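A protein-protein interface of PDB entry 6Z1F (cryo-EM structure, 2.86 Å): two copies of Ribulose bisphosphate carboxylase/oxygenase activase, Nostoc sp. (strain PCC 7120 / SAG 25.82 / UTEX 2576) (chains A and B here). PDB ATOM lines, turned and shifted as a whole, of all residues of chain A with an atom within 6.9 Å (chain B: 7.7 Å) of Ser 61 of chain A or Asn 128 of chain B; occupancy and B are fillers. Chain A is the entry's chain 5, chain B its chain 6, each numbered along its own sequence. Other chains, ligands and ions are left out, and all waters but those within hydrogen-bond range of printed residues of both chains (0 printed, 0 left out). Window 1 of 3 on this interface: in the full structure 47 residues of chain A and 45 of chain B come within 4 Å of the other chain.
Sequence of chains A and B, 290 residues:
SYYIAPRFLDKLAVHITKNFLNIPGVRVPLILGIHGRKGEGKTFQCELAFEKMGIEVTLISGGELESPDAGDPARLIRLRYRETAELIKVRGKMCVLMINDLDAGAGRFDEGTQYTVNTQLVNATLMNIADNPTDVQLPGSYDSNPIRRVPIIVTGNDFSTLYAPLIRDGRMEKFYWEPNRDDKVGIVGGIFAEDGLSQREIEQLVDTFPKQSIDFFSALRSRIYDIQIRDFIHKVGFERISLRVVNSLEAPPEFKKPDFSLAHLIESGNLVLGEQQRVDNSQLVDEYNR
OG of Ser 61 of chain A lies within hydrogen-bond range of ND2 of Asn 128 of chain B (2.8 Å). The backbone carbonyl oxygen of Asn 100 of chain A is in hydrogen-bond range of the side-chain amide nitrogen of Asn 128 of chain B, at 3.5 Å. The backbone carbonyl oxygen (O) of Gly 63 of chain A lies within hydrogen-bond range of the side-chain hydroxyl (OG1) of Thr 125 of chain B, 3.4 Å away. NH1 of Arg 78 of chain B lies within hydrogen-bond range of O of Gly 63 of chain A (2.8 Å). The backbone NH (N) of Gly 62 of chain A lies close to the side-chain amide nitrogen (ND2) of Asn 128 of chain B, 3.4 Å away. The side-chain carboxylate of Glu 64 of chain A is in salt-bridge range of the guanidinium group of Arg 78 of chain B, 3.98 Å away.
The backbone carbonyl oxygen of Ile 60 of chain A sits at hydrogen-bond distance from the backbone NH of Asn 100 of chain A (3.4 Å). O of Leu 121 of chain B lies within hydrogen-bond range of OG1 of Thr 125 of chain B (2.8 Å). OD1 of Asp 131 of chain B lies within salt-bridge range of NH1 of Arg 171 of chain B, at 2.8 Å. The backbone carbonyl oxygen of Ala 124 of chain B lies close to the side-chain amide oxygen of Asn 128 of chain B, at 3.0 Å. The backbone carbonyl oxygen (O) of Met 127 of chain B lies within hydrogen-bond range of the guanidinium group (NH1) of Arg 171 of chain B, 3.0 Å away. The side-chain hydroxyl of Ser 61 of chain A lies close to the backbone NH of Gly 63 of chain A.
CD1 of Leu 59 of chain A touches ND2 of Asn 132 of chain B, 3.7 Å away. Gly 63 of chain A touches Leu 121 of chain B. Ala 124 of chain B touches Gly 63 of chain A. Asp 131 of chain B touches Asn 100 of chain A (OD2 to ND2, 3.8 Å). Asp 101 of chain A touches Met 127 of chain B (OD2 to CE, 3.4 Å).
Of chain A, only Ser 61 (2.8 Å), Gly 62 (3.4 Å) and Asn 100 (3.5 Å) come within 4 Å of Asn 128 of chain B. Of the printed residues of chain A, Thr 125 of chain B touches Gly 63 (3.4 Å). Printed residues of chain B within 4 Å of Asp 101 of chain A: Met 127 (3.4 Å). Printed residues of chain A within 4 Å of Ala 124 of chain B: Gly 63 (3.9 Å). Of the printed residues of chain A, Asp 131 of chain B touches Asn 100 (3.8 Å). Of the printed residues of chain A, Leu 121 of chain B touches Gly 63 (3.9 Å). Leu 166 of chain B touches none of the printed residues of chain A. Leu 76 of chain A touches none of the printed residues of chain B. The nearest residue of chain B that does not touch Ser 61 of chain A is Arg 78 of chain B (4.2 Å).
Hydrophobic or aromatic side chains of chain A within 4 Å of the printed part of chain B: Leu 59. Among the printed residues, 11 pairs touch across the chains. Among the printed residues, Asp or Glu carboxylates within 4 Å of a Lys or Arg side-chain nitrogen of the other chain: Glu 64 of chain A with Arg 78 of chain B (3.98 Å).
No position is printed for both chains.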
ATOM      1  N   LEU A  59     -21.467 -13.608  29.848  1.00  0.00           N
ATOM      2  CA  LEU A  59     -20.545 -12.540  29.495  1.00  0.00           C
ATOM      3  C   LEU A  59     -19.604 -12.231  30.655  1.00  0.00           C
ATOM      4  O   LEU A  59     -20.041 -12.081  31.796  1.00  0.00           O
ATOM      5  CB  LEU A  59     -21.337 -11.296  29.078  1.00  0.00           C
ATOM      6  CG  LEU A  59     -21.907 -11.313  27.658  1.00  0.00           C
ATOM      7  CD1 LEU A  59     -23.000 -10.263  27.494  1.00  0.00           C
ATOM      8  CD2 LEU A  59     -20.807 -11.091  26.629  1.00  0.00           C
ATOM      9  N   ILE A  60     -18.309 -12.142  30.330  1.00  0.00           N
ATOM     10  CA  ILE A  60     -17.262 -11.701  31.239  1.00  0.00           C
ATOM     11  C   ILE A  60     -16.643 -10.441  30.641  1.00  0.00           C
ATOM     12  O   ILE A  60     -16.260 -10.436  29.469  1.00  0.00           O
ATOM     13  CB  ILE A  60     -16.210 -12.811  31.437  1.00  0.00           C
ATOM     14  CG1 ILE A  60     -16.816 -14.069  32.064  1.00  0.00           C
ATOM     15  CG2 ILE A  60     -15.026 -12.296  32.239  1.00  0.00           C
ATOM     16  CD1 ILE A  60     -15.922 -15.291  32.028  1.00  0.00           C
ATOM     17  N   SER A  61     -16.559  -9.377  31.448  1.00  0.00           N
ATOM     18  CA  SER A  61     -15.963  -8.131  30.990  1.00  0.00           C
ATOM     19  C   SER A  61     -14.443  -8.199  31.110  1.00  0.00           C
ATOM     20  O   SER A  61     -13.921  -8.720  32.093  1.00  0.00           O
ATOM     21  CB  SER A  61     -16.518  -6.935  31.717  1.00  0.00           C
ATOM     22  OG  SER A  61     -15.932  -5.733  31.229  1.00  0.00           O
ATOM     23  N   GLY A  62     -13.756  -7.650  30.103  1.00  0.00           N
ATOM     24  CA  GLY A  62     -12.304  -7.613  30.063  1.00  0.00           C
ATOM     25  C   GLY A  62     -11.717  -6.741  31.172  1.00  0.00           C
ATOM     26  O   GLY A  62     -10.604  -6.990  31.636  1.00  0.00           O
ATOM     27  N   GLY A  63     -12.486  -5.727  31.589  1.00  0.00           N
ATOM     28  CA  GLY A  63     -12.095  -4.833  32.665  1.00  0.00           C
ATOM     29  C   GLY A  63     -12.553  -5.349  34.025  1.00  0.00           C
ATOM     30  O   GLY A  63     -12.869  -4.557  34.910  1.00  0.00           O
ATOM     31  N   GLU A  64     -12.574  -6.677  34.175  1.00  0.00           N
ATOM     32  CA  GLU A  64     -12.967  -7.330  35.412  1.00  0.00           C
ATOM     33  C   GLU A  64     -11.914  -8.368  35.799  1.00  0.00           C
ATOM     34  O   GLU A  64     -12.034  -9.029  36.829  1.00  0.00           O
ATOM     35  CB  GLU A  64     -14.357  -7.950  35.246  1.00  0.00           C
ATOM     36  CG  GLU A  64     -15.130  -8.053  36.549  1.00  0.00           C
ATOM     37  CD  GLU A  64     -16.587  -8.474  36.441  1.00  0.00           C
ATOM     38  OE1 GLU A  64     -17.298  -7.944  35.556  1.00  0.00           O
ATOM     39  OE2 GLU A  64     -17.015  -9.325  37.252  1.00  0.00           O
ATOM     40  N   LEU A  65     -10.864  -8.474  34.972  1.00  0.00           N
ATOM     41  CA  LEU A  65      -9.846  -9.505  35.116  1.00  0.00           C
ATOM     42  C   LEU A  65      -8.636  -8.955  35.874  1.00  0.00           C
ATOM     43  O   LEU A  65      -7.490  -9.225  35.508  1.00  0.00           O
ATOM     44  CB  LEU A  65      -9.465 -10.030  33.725  1.00  0.00           C
ATOM     45  CG  LEU A  65     -10.596 -10.621  32.881  1.00  0.00           C
ATOM     46  CD1 LEU A  65     -10.144 -10.834  31.444  1.00  0.00           C
ATOM     47  CD2 LEU A  65     -11.117 -11.926  33.468  1.00  0.00           C
ATOM     48  N   LEU A  76     -12.971 -16.336  39.369  1.00  0.00           N
ATOM     49  CA  LEU A  76     -14.157 -15.883  38.657  1.00  0.00           C
ATOM     50  C   LEU A  76     -14.383 -16.712  37.394  1.00  0.00           C
ATOM     51  O   LEU A  76     -15.504 -17.159  37.152  1.00  0.00           O
ATOM     52  CB  LEU A  76     -14.030 -14.390  38.331  1.00  0.00           C
ATOM     53  CG  LEU A  76     -15.237 -13.762  37.631  1.00  0.00           C
ATOM     54  CD1 LEU A  76     -16.343 -13.446  38.628  1.00  0.00           C
ATOM     55  CD2 LEU A  76     -14.845 -12.511  36.855  1.00  0.00           C
ATOM     56  N   MET A  98     -18.378 -15.993  26.733  1.00  0.00           N
ATOM     57  CA  MET A  98     -17.735 -14.957  25.938  1.00  0.00           C
ATOM     58  C   MET A  98     -17.002 -13.973  26.846  1.00  0.00           C
ATOM     59  O   MET A  98     -17.611 -13.367  27.725  1.00  0.00           O
ATOM     60  CB  MET A  98     -18.741 -14.204  25.059  1.00  0.00           C
ATOM     61  CG  MET A  98     -18.082 -13.158  24.163  1.00  0.00           C
ATOM     62  SD  MET A  98     -18.905 -12.862  22.568  1.00  0.00           S
ATOM     63  CE  MET A  98     -20.169 -11.682  23.044  1.00  0.00           C
ATOM     64  N   ILE A  99     -15.690 -13.831  26.612  1.00  0.00           N
ATOM     65  CA  ILE A  99     -14.899 -12.764  27.209  1.00  0.00           C
ATOM     66  C   ILE A  99     -14.608 -11.720  26.130  1.00  0.00           C
ATOM     67  O   ILE A  99     -13.785 -11.939  25.241  1.00  0.00           O
ATOM     68  CB  ILE A  99     -13.617 -13.281  27.905  1.00  0.00           C
ATOM     69  CG1 ILE A  99     -13.909 -14.387  28.924  1.00  0.00           C
ATOM     70  CG2 ILE A  99     -12.848 -12.127  28.541  1.00  0.00           C
ATOM     71  CD1 ILE A  99     -12.723 -15.285  29.231  1.00  0.00           C
ATOM     72  N   ASN A 100     -15.314 -10.588  26.235  1.00  0.00           N
ATOM     73  CA  ASN A 100     -15.178  -9.465  25.325  1.00  0.00           C
ATOM     74  C   ASN A 100     -14.027  -8.580  25.795  1.00  0.00           C
ATOM     75  O   ASN A 100     -13.991  -8.170  26.955  1.00  0.00           O
ATOM     76  CB  ASN A 100     -16.489  -8.684  25.215  1.00  0.00           C
ATOM     77  CG  ASN A 100     -16.428  -7.555  24.212  1.00  0.00           C
ATOM     78  OD1 ASN A 100     -16.194  -7.783  23.027  1.00  0.00           O
ATOM     79  ND2 ASN A 100     -16.644  -6.334  24.676  1.00  0.00           N
ATOM     80  N   ASP A 101     -13.093  -8.317  24.871  1.00  0.00           N
ATOM     81  CA  ASP A 101     -11.954  -7.424  25.044  1.00  0.00           C
ATOM     82  C   ASP A 101     -10.943  -8.034  26.015  1.00  0.00           C
ATOM     83  O   ASP A 101     -10.782  -7.558  27.136  1.00  0.00           O
ATOM     84  CB  ASP A 101     -12.392  -5.992  25.371  1.00  0.00           C
ATOM     85  CG  ASP A 101     -11.281  -4.973  25.198  1.00  0.00           C
ATOM     86  OD1 ASP A 101     -10.983  -4.622  24.038  1.00  0.00           O
ATOM     87  OD2 ASP A 101     -10.718  -4.545  26.226  1.00  0.00           O
ATOM     88  N   GLY A 105      -7.286  -6.956  29.259  1.00  0.00           N
ATOM     89  CA  GLY A 105      -7.396  -7.739  30.480  1.00  0.00           C
ATOM     90  C   GLY A 105      -6.056  -8.354  30.873  1.00  0.00           C
ATOM     91  O   GLY A 105      -5.442  -7.936  31.854  1.00  0.00           O
ATOM     92  N   LEU B  30     -23.832   5.944  24.119  1.00  0.00           N
ATOM     93  CA  LEU B  30     -24.164   5.992  25.534  1.00  0.00           C
ATOM     94  C   LEU B  30     -23.341   7.061  26.248  1.00  0.00           C
ATOM     95  O   LEU B  30     -23.693   7.463  27.354  1.00  0.00           O
ATOM     96  CB  LEU B  30     -23.912   4.613  26.151  1.00  0.00           C
ATOM     97  CG  LEU B  30     -24.506   4.390  27.543  1.00  0.00           C
ATOM     98  CD1 LEU B  30     -25.981   4.016  27.463  1.00  0.00           C
ATOM     99  CD2 LEU B  30     -23.726   3.335  28.315  1.00  0.00           C
ATOM    100  N   ARG B  78     -18.413   0.272  38.013  1.00  0.00           N
ATOM    101  CA  ARG B  78     -19.460  -0.732  37.901  1.00  0.00           C
ATOM    102  C   ARG B  78     -20.431  -0.632  39.075  1.00  0.00           C
ATOM    103  O   ARG B  78     -21.630  -0.843  38.902  1.00  0.00           O
ATOM    104  CB  ARG B  78     -18.861  -2.136  37.824  1.00  0.00           C
ATOM    105  CG  ARG B  78     -18.492  -2.570  36.415  1.00  0.00           C
ATOM    106  CD  ARG B  78     -18.106  -4.034  36.366  1.00  0.00           C
ATOM    107  NE  ARG B  78     -16.840  -4.274  37.037  1.00  0.00           N
ATOM    108  CZ  ARG B  78     -15.661  -4.308  36.431  1.00  0.00           C
ATOM    109  NH1 ARG B  78     -15.580  -4.132  35.124  1.00  0.00           N
ATOM    110  NH2 ARG B  78     -14.566  -4.527  37.137  1.00  0.00           N
ATOM    111  N   LEU B 121      -7.354  -0.674  32.645  1.00  0.00           N
ATOM    112  CA  LEU B 121      -8.608  -1.236  33.130  1.00  0.00           C
ATOM    113  C   LEU B 121      -9.751  -0.228  33.041  1.00  0.00           C
ATOM    114  O   LEU B 121     -10.889  -0.614  32.782  1.00  0.00           O
ATOM    115  CB  LEU B 121      -8.439  -1.694  34.580  1.00  0.00           C
ATOM    116  CG  LEU B 121      -7.744  -3.036  34.787  1.00  0.00           C
ATOM    117  CD1 LEU B 121      -7.322  -3.180  36.240  1.00  0.00           C
ATOM    118  CD2 LEU B 121      -8.642  -4.196  34.381  1.00  0.00           C
ATOM    119  N   VAL B 122      -9.450   1.050  33.299  1.00  0.00           N
ATOM    120  CA  VAL B 122     -10.462   2.093  33.301  1.00  0.00           C
ATOM    121  C   VAL B 122     -10.992   2.284  31.878  1.00  0.00           C
ATOM    122  O   VAL B 122     -12.196   2.455  31.682  1.00  0.00           O
ATOM    123  CB  VAL B 122      -9.937   3.387  33.955  1.00  0.00           C
ATOM    124  CG1 VAL B 122     -10.643   4.643  33.465  1.00  0.00           C
ATOM    125  CG2 VAL B 122     -10.016   3.301  35.470  1.00  0.00           C
ATOM    126  N   ASN B 123     -10.086   2.209  30.897  1.00  0.00           N
ATOM    127  CA  ASN B 123     -10.449   2.269  29.490  1.00  0.00           C
ATOM    128  C   ASN B 123     -11.270   1.040  29.100  1.00  0.00           C
ATOM    129  O   ASN B 123     -12.226   1.156  28.334  1.00  0.00           O
ATOM    130  CB  ASN B 123      -9.224   2.457  28.595  1.00  0.00           C
ATOM    131  CG  ASN B 123      -8.755   3.896  28.543  1.00  0.00           C
ATOM    132  OD1 ASN B 123      -7.879   4.299  29.306  1.00  0.00           O
ATOM    133  ND2 ASN B 123      -9.337   4.682  27.653  1.00  0.00           N
ATOM    134  N   ALA B 124     -10.890  -0.126  29.641  1.00  0.00           N
ATOM    135  CA  ALA B 124     -11.505  -1.398  29.293  1.00  0.00           C
ATOM    136  C   ALA B 124     -12.951  -1.449  29.780  1.00  0.00           C
ATOM    137  O   ALA B 124     -13.816  -1.940  29.061  1.00  0.00           O
ATOM    138  CB  ALA B 124     -10.695  -2.543  29.849  1.00  0.00           C
ATOM    139  N   THR B 125     -13.184  -0.936  30.997  1.00  0.00           N
ATOM    140  CA  THR B 125     -14.472  -1.017  31.670  1.00  0.00           C
ATOM    141  C   THR B 125     -15.512  -0.194  30.915  1.00  0.00           C
ATOM    142  O   THR B 125     -16.598  -0.696  30.626  1.00  0.00           O
ATOM    143  CB  THR B 125     -14.360  -0.614  33.146  1.00  0.00           C
ATOM    144  OG1 THR B 125     -13.369  -1.440  33.758  1.00  0.00           O
ATOM    145  CG2 THR B 125     -15.671  -0.752  33.890  1.00  0.00           C
ATOM    146  N   LEU B 126     -15.153   1.052  30.579  1.00  0.00           N
ATOM    147  CA  LEU B 126     -16.055   2.000  29.941  1.00  0.00           C
ATOM    148  C   LEU B 126     -16.479   1.520  28.552  1.00  0.00           C
ATOM    149  O   LEU B 126     -17.550   1.896  28.077  1.00  0.00           O
ATOM    150  CB  LEU B 126     -15.380   3.375  29.876  1.00  0.00           C
ATOM    151  CG  LEU B 126     -15.470   4.213  31.151  1.00  0.00           C
ATOM    152  CD1 LEU B 126     -14.411   5.304  31.162  1.00  0.00           C
ATOM    153  CD2 LEU B 126     -16.857   4.823  31.312  1.00  0.00           C
ATOM    154  N   MET B 127     -15.632   0.698  27.915  1.00  0.00           N
ATOM    155  CA  MET B 127     -15.903   0.122  26.608  1.00  0.00           C
ATOM    156  C   MET B 127     -17.042  -0.888  26.705  1.00  0.00           C
ATOM    157  O   MET B 127     -17.922  -0.912  25.848  1.00  0.00           O
ATOM    158  CB  MET B 127     -14.666  -0.602  26.077  1.00  0.00           C
ATOM    159  CG  MET B 127     -13.741   0.260  25.252  1.00  0.00           C
ATOM    160  SD  MET B 127     -12.608  -0.784  24.286  1.00  0.00           S
ATOM    161  CE  MET B 127     -11.415  -1.243  25.543  1.00  0.00           C
ATOM    162  N   ASN B 128     -17.009  -1.710  27.761  1.00  0.00           N
ATOM    163  CA  ASN B 128     -17.903  -2.845  27.924  1.00  0.00           C
ATOM    164  C   ASN B 128     -19.285  -2.393  28.392  1.00  0.00           C
ATOM    165  O   ASN B 128     -20.280  -3.040  28.069  1.00  0.00           O
ATOM    166  CB  ASN B 128     -17.311  -3.886  28.877  1.00  0.00           C
ATOM    167  CG  ASN B 128     -16.182  -4.685  28.262  1.00  0.00           C
ATOM    168  OD1 ASN B 128     -15.299  -4.135  27.604  1.00  0.00           O
ATOM    169  ND2 ASN B 128     -16.202  -5.990  28.475  1.00  0.00           N
ATOM    170  N   ILE B 129     -19.331  -1.304  29.172  1.00  0.00           N
ATOM    171  CA  ILE B 129     -20.590  -0.727  29.619  1.00  0.00           C
ATOM    172  C   ILE B 129     -21.306  -0.131  28.408  1.00  0.00           C
ATOM    173  O   ILE B 129     -22.519  -0.270  28.277  1.00  0.00           O
ATOM    174  CB  ILE B 129     -20.388   0.293  30.762  1.00  0.00           C
ATOM    175  CG1 ILE B 129     -19.618  -0.317  31.939  1.00  0.00           C
ATOM    176  CG2 ILE B 129     -21.723   0.867  31.221  1.00  0.00           C
ATOM    177  CD1 ILE B 129     -19.109   0.688  32.958  1.00  0.00           C
ATOM    178  N   ALA B 130     -20.531   0.495  27.511  1.00  0.00           N
ATOM    179  CA  ALA B 130     -21.048   1.138  26.313  1.00  0.00           C
ATOM    180  C   ALA B 130     -21.528   0.107  25.290  1.00  0.00           C
ATOM    181  O   ALA B 130     -22.343   0.432  24.428  1.00  0.00           O
ATOM    182  CB  ALA B 130     -20.001   2.061  25.743  1.00  0.00           C
ATOM    183  N   ASP B 131     -21.025  -1.132  25.397  1.00  0.00           N
ATOM    184  CA  ASP B 131     -21.426  -2.225  24.524  1.00  0.00           C
ATOM    185  C   ASP B 131     -22.655  -2.936  25.088  1.00  0.00           C
ATOM    186  O   ASP B 131     -23.599  -3.206  24.349  1.00  0.00           O
ATOM    187  CB  ASP B 131     -20.271  -3.197  24.252  1.00  0.00           C
ATOM    188  CG  ASP B 131     -19.386  -2.814  23.071  1.00  0.00           C
ATOM    189  OD1 ASP B 131     -19.542  -1.683  22.549  1.00  0.00           O
ATOM    190  OD2 ASP B 131     -18.540  -3.651  22.679  1.00  0.00           O
ATOM    191  N   ASN B 132     -22.621  -3.245  26.392  1.00  0.00           N
ATOM    192  CA  ASN B 132     -23.719  -3.909  27.081  1.00  0.00           C
ATOM    193  C   ASN B 132     -24.190  -3.042  28.248  1.00  0.00           C
ATOM    194  O   ASN B 132     -23.750  -3.246  29.381  1.00  0.00           O
ATOM    195  CB  ASN B 132     -23.335  -5.312  27.559  1.00  0.00           C
ATOM    196  CG  ASN B 132     -23.191  -6.320  26.437  1.00  0.00           C
ATOM    197  OD1 ASN B 132     -24.134  -6.557  25.683  1.00  0.00           O
ATOM    198  ND2 ASN B 132     -22.022  -6.933  26.334  1.00  0.00           N
ATOM    199  N   PRO B 133     -25.092  -2.054  28.019  1.00  0.00           N
ATOM    200  CA  PRO B 133     -25.602  -1.206  29.099  1.00  0.00           C
ATOM    201  C   PRO B 133     -26.572  -1.946  30.015  1.00  0.00           C
ATOM    202  O   PRO B 133     -26.801  -1.517  31.145  1.00  0.00           O
ATOM    203  CB  PRO B 133     -26.320  -0.061  28.366  1.00  0.00           C
ATOM    204  CG  PRO B 133     -25.891  -0.190  26.918  1.00  0.00           C
ATOM    205  CD  PRO B 133     -25.653  -1.670  26.713  1.00  0.00           C
ATOM    206  N   THR B 134     -27.113  -3.065  29.514  1.00  0.00           N
ATOM    207  CA  THR B 134     -28.147  -3.836  30.190  1.00  0.00           C
ATOM    208  C   THR B 134     -27.537  -4.994  30.983  1.00  0.00           C
ATOM    209  O   THR B 134     -28.232  -5.613  31.788  1.00  0.00           O
ATOM    210  CB  THR B 134     -29.227  -4.306  29.207  1.00  0.00           C
ATOM    211  OG1 THR B 134     -28.585  -4.705  27.996  1.00  0.00           O
ATOM    212  CG2 THR B 134     -30.246  -3.234  28.890  1.00  0.00           C
ATOM    213  N   ASP B 135     -26.242  -5.268  30.760  1.00  0.00           N
ATOM    214  CA  ASP B 135     -25.588  -6.429  31.346  1.00  0.00           C
ATOM    215  C   ASP B 135     -24.274  -6.020  32.013  1.00  0.00           C
ATOM    216  O   ASP B 135     -23.201  -6.174  31.432  1.00  0.00           O
ATOM    217  CB  ASP B 135     -25.424  -7.552  30.313  1.00  0.00           C
ATOM    218  CG  ASP B 135     -25.225  -8.939  30.912  1.00  0.00           C
ATOM    219  OD1 ASP B 135     -24.210  -9.143  31.621  1.00  0.00           O
ATOM    220  OD2 ASP B 135     -26.088  -9.810  30.662  1.00  0.00           O
ATOM    221  N   VAL B 136     -24.381  -5.506  33.242  1.00  0.00           N
ATOM    222  CA  VAL B 136     -23.230  -5.138  34.053  1.00  0.00           C
ATOM    223  C   VAL B 136     -23.255  -6.015  35.299  1.00  0.00           C
ATOM    224  O   VAL B 136     -24.278  -6.089  35.979  1.00  0.00           O
ATOM    225  CB  VAL B 136     -23.237  -3.637  34.411  1.00  0.00           C
ATOM    226  CG1 VAL B 136     -22.142  -3.271  35.403  1.00  0.00           C
ATOM    227  CG2 VAL B 136     -23.146  -2.748  33.180  1.00  0.00           C
ATOM    228  N   GLN B 137     -22.120  -6.666  35.589  1.00  0.00           N
ATOM    229  CA  GLN B 137     -22.058  -7.655  36.655  1.00  0.00           C
ATOM    230  C   GLN B 137     -21.392  -7.081  37.900  1.00  0.00           C
ATOM    231  O   GLN B 137     -20.435  -6.316  37.815  1.00  0.00           O
ATOM    232  CB  GLN B 137     -21.340  -8.927  36.201  1.00  0.00           C
ATOM    233  CG  GLN B 137     -22.173  -9.816  35.285  1.00  0.00           C
ATOM    234  CD  GLN B 137     -23.457 -10.324  35.898  1.00  0.00           C
ATOM    235  OE1 GLN B 137     -23.528 -10.628  37.088  1.00  0.00           O
ATOM    236  NE2 GLN B 137     -24.485 -10.429  35.073  1.00  0.00           N
ATOM    237  N   LEU B 166     -12.083   3.651  22.589  1.00  0.00           N
ATOM    238  CA  LEU B 166     -13.045   4.315  23.458  1.00  0.00           C
ATOM    239  C   LEU B 166     -13.588   5.580  22.792  1.00  0.00           C
ATOM    240  O   LEU B 166     -14.671   6.050  23.140  1.00  0.00           O
ATOM    241  CB  LEU B 166     -12.396   4.609  24.816  1.00  0.00           C
ATOM    242  CG  LEU B 166     -13.308   5.162  25.917  1.00  0.00           C
ATOM    243  CD1 LEU B 166     -14.467   4.227  26.226  1.00  0.00           C
ATOM    244  CD2 LEU B 166     -12.516   5.435  27.182  1.00  0.00           C
ATOM    245  N   ARG B 171     -19.568   4.819  19.720  1.00  0.00           N
ATOM    246  CA  ARG B 171     -19.426   4.581  21.150  1.00  0.00           C
ATOM    247  C   ARG B 171     -19.508   5.885  21.940  1.00  0.00           C
ATOM    248  O   ARG B 171     -19.852   5.867  23.120  1.00  0.00           O
ATOM    249  CB  ARG B 171     -18.107   3.863  21.445  1.00  0.00           C
ATOM    250  CG  ARG B 171     -18.217   2.798  22.524  1.00  0.00           C
ATOM    251  CD  ARG B 171     -16.865   2.409  23.084  1.00  0.00           C
ATOM    252  NE  ARG B 171     -16.105   1.492  22.244  1.00  0.00           N
ATOM    253  CZ  ARG B 171     -16.233   0.169  22.247  1.00  0.00           C
ATOM    254  NH1 ARG B 171     -17.111  -0.416  23.043  1.00  0.00           N
ATOM    255  NH2 ARG B 171     -15.487  -0.567  21.445  1.00  0.00           N
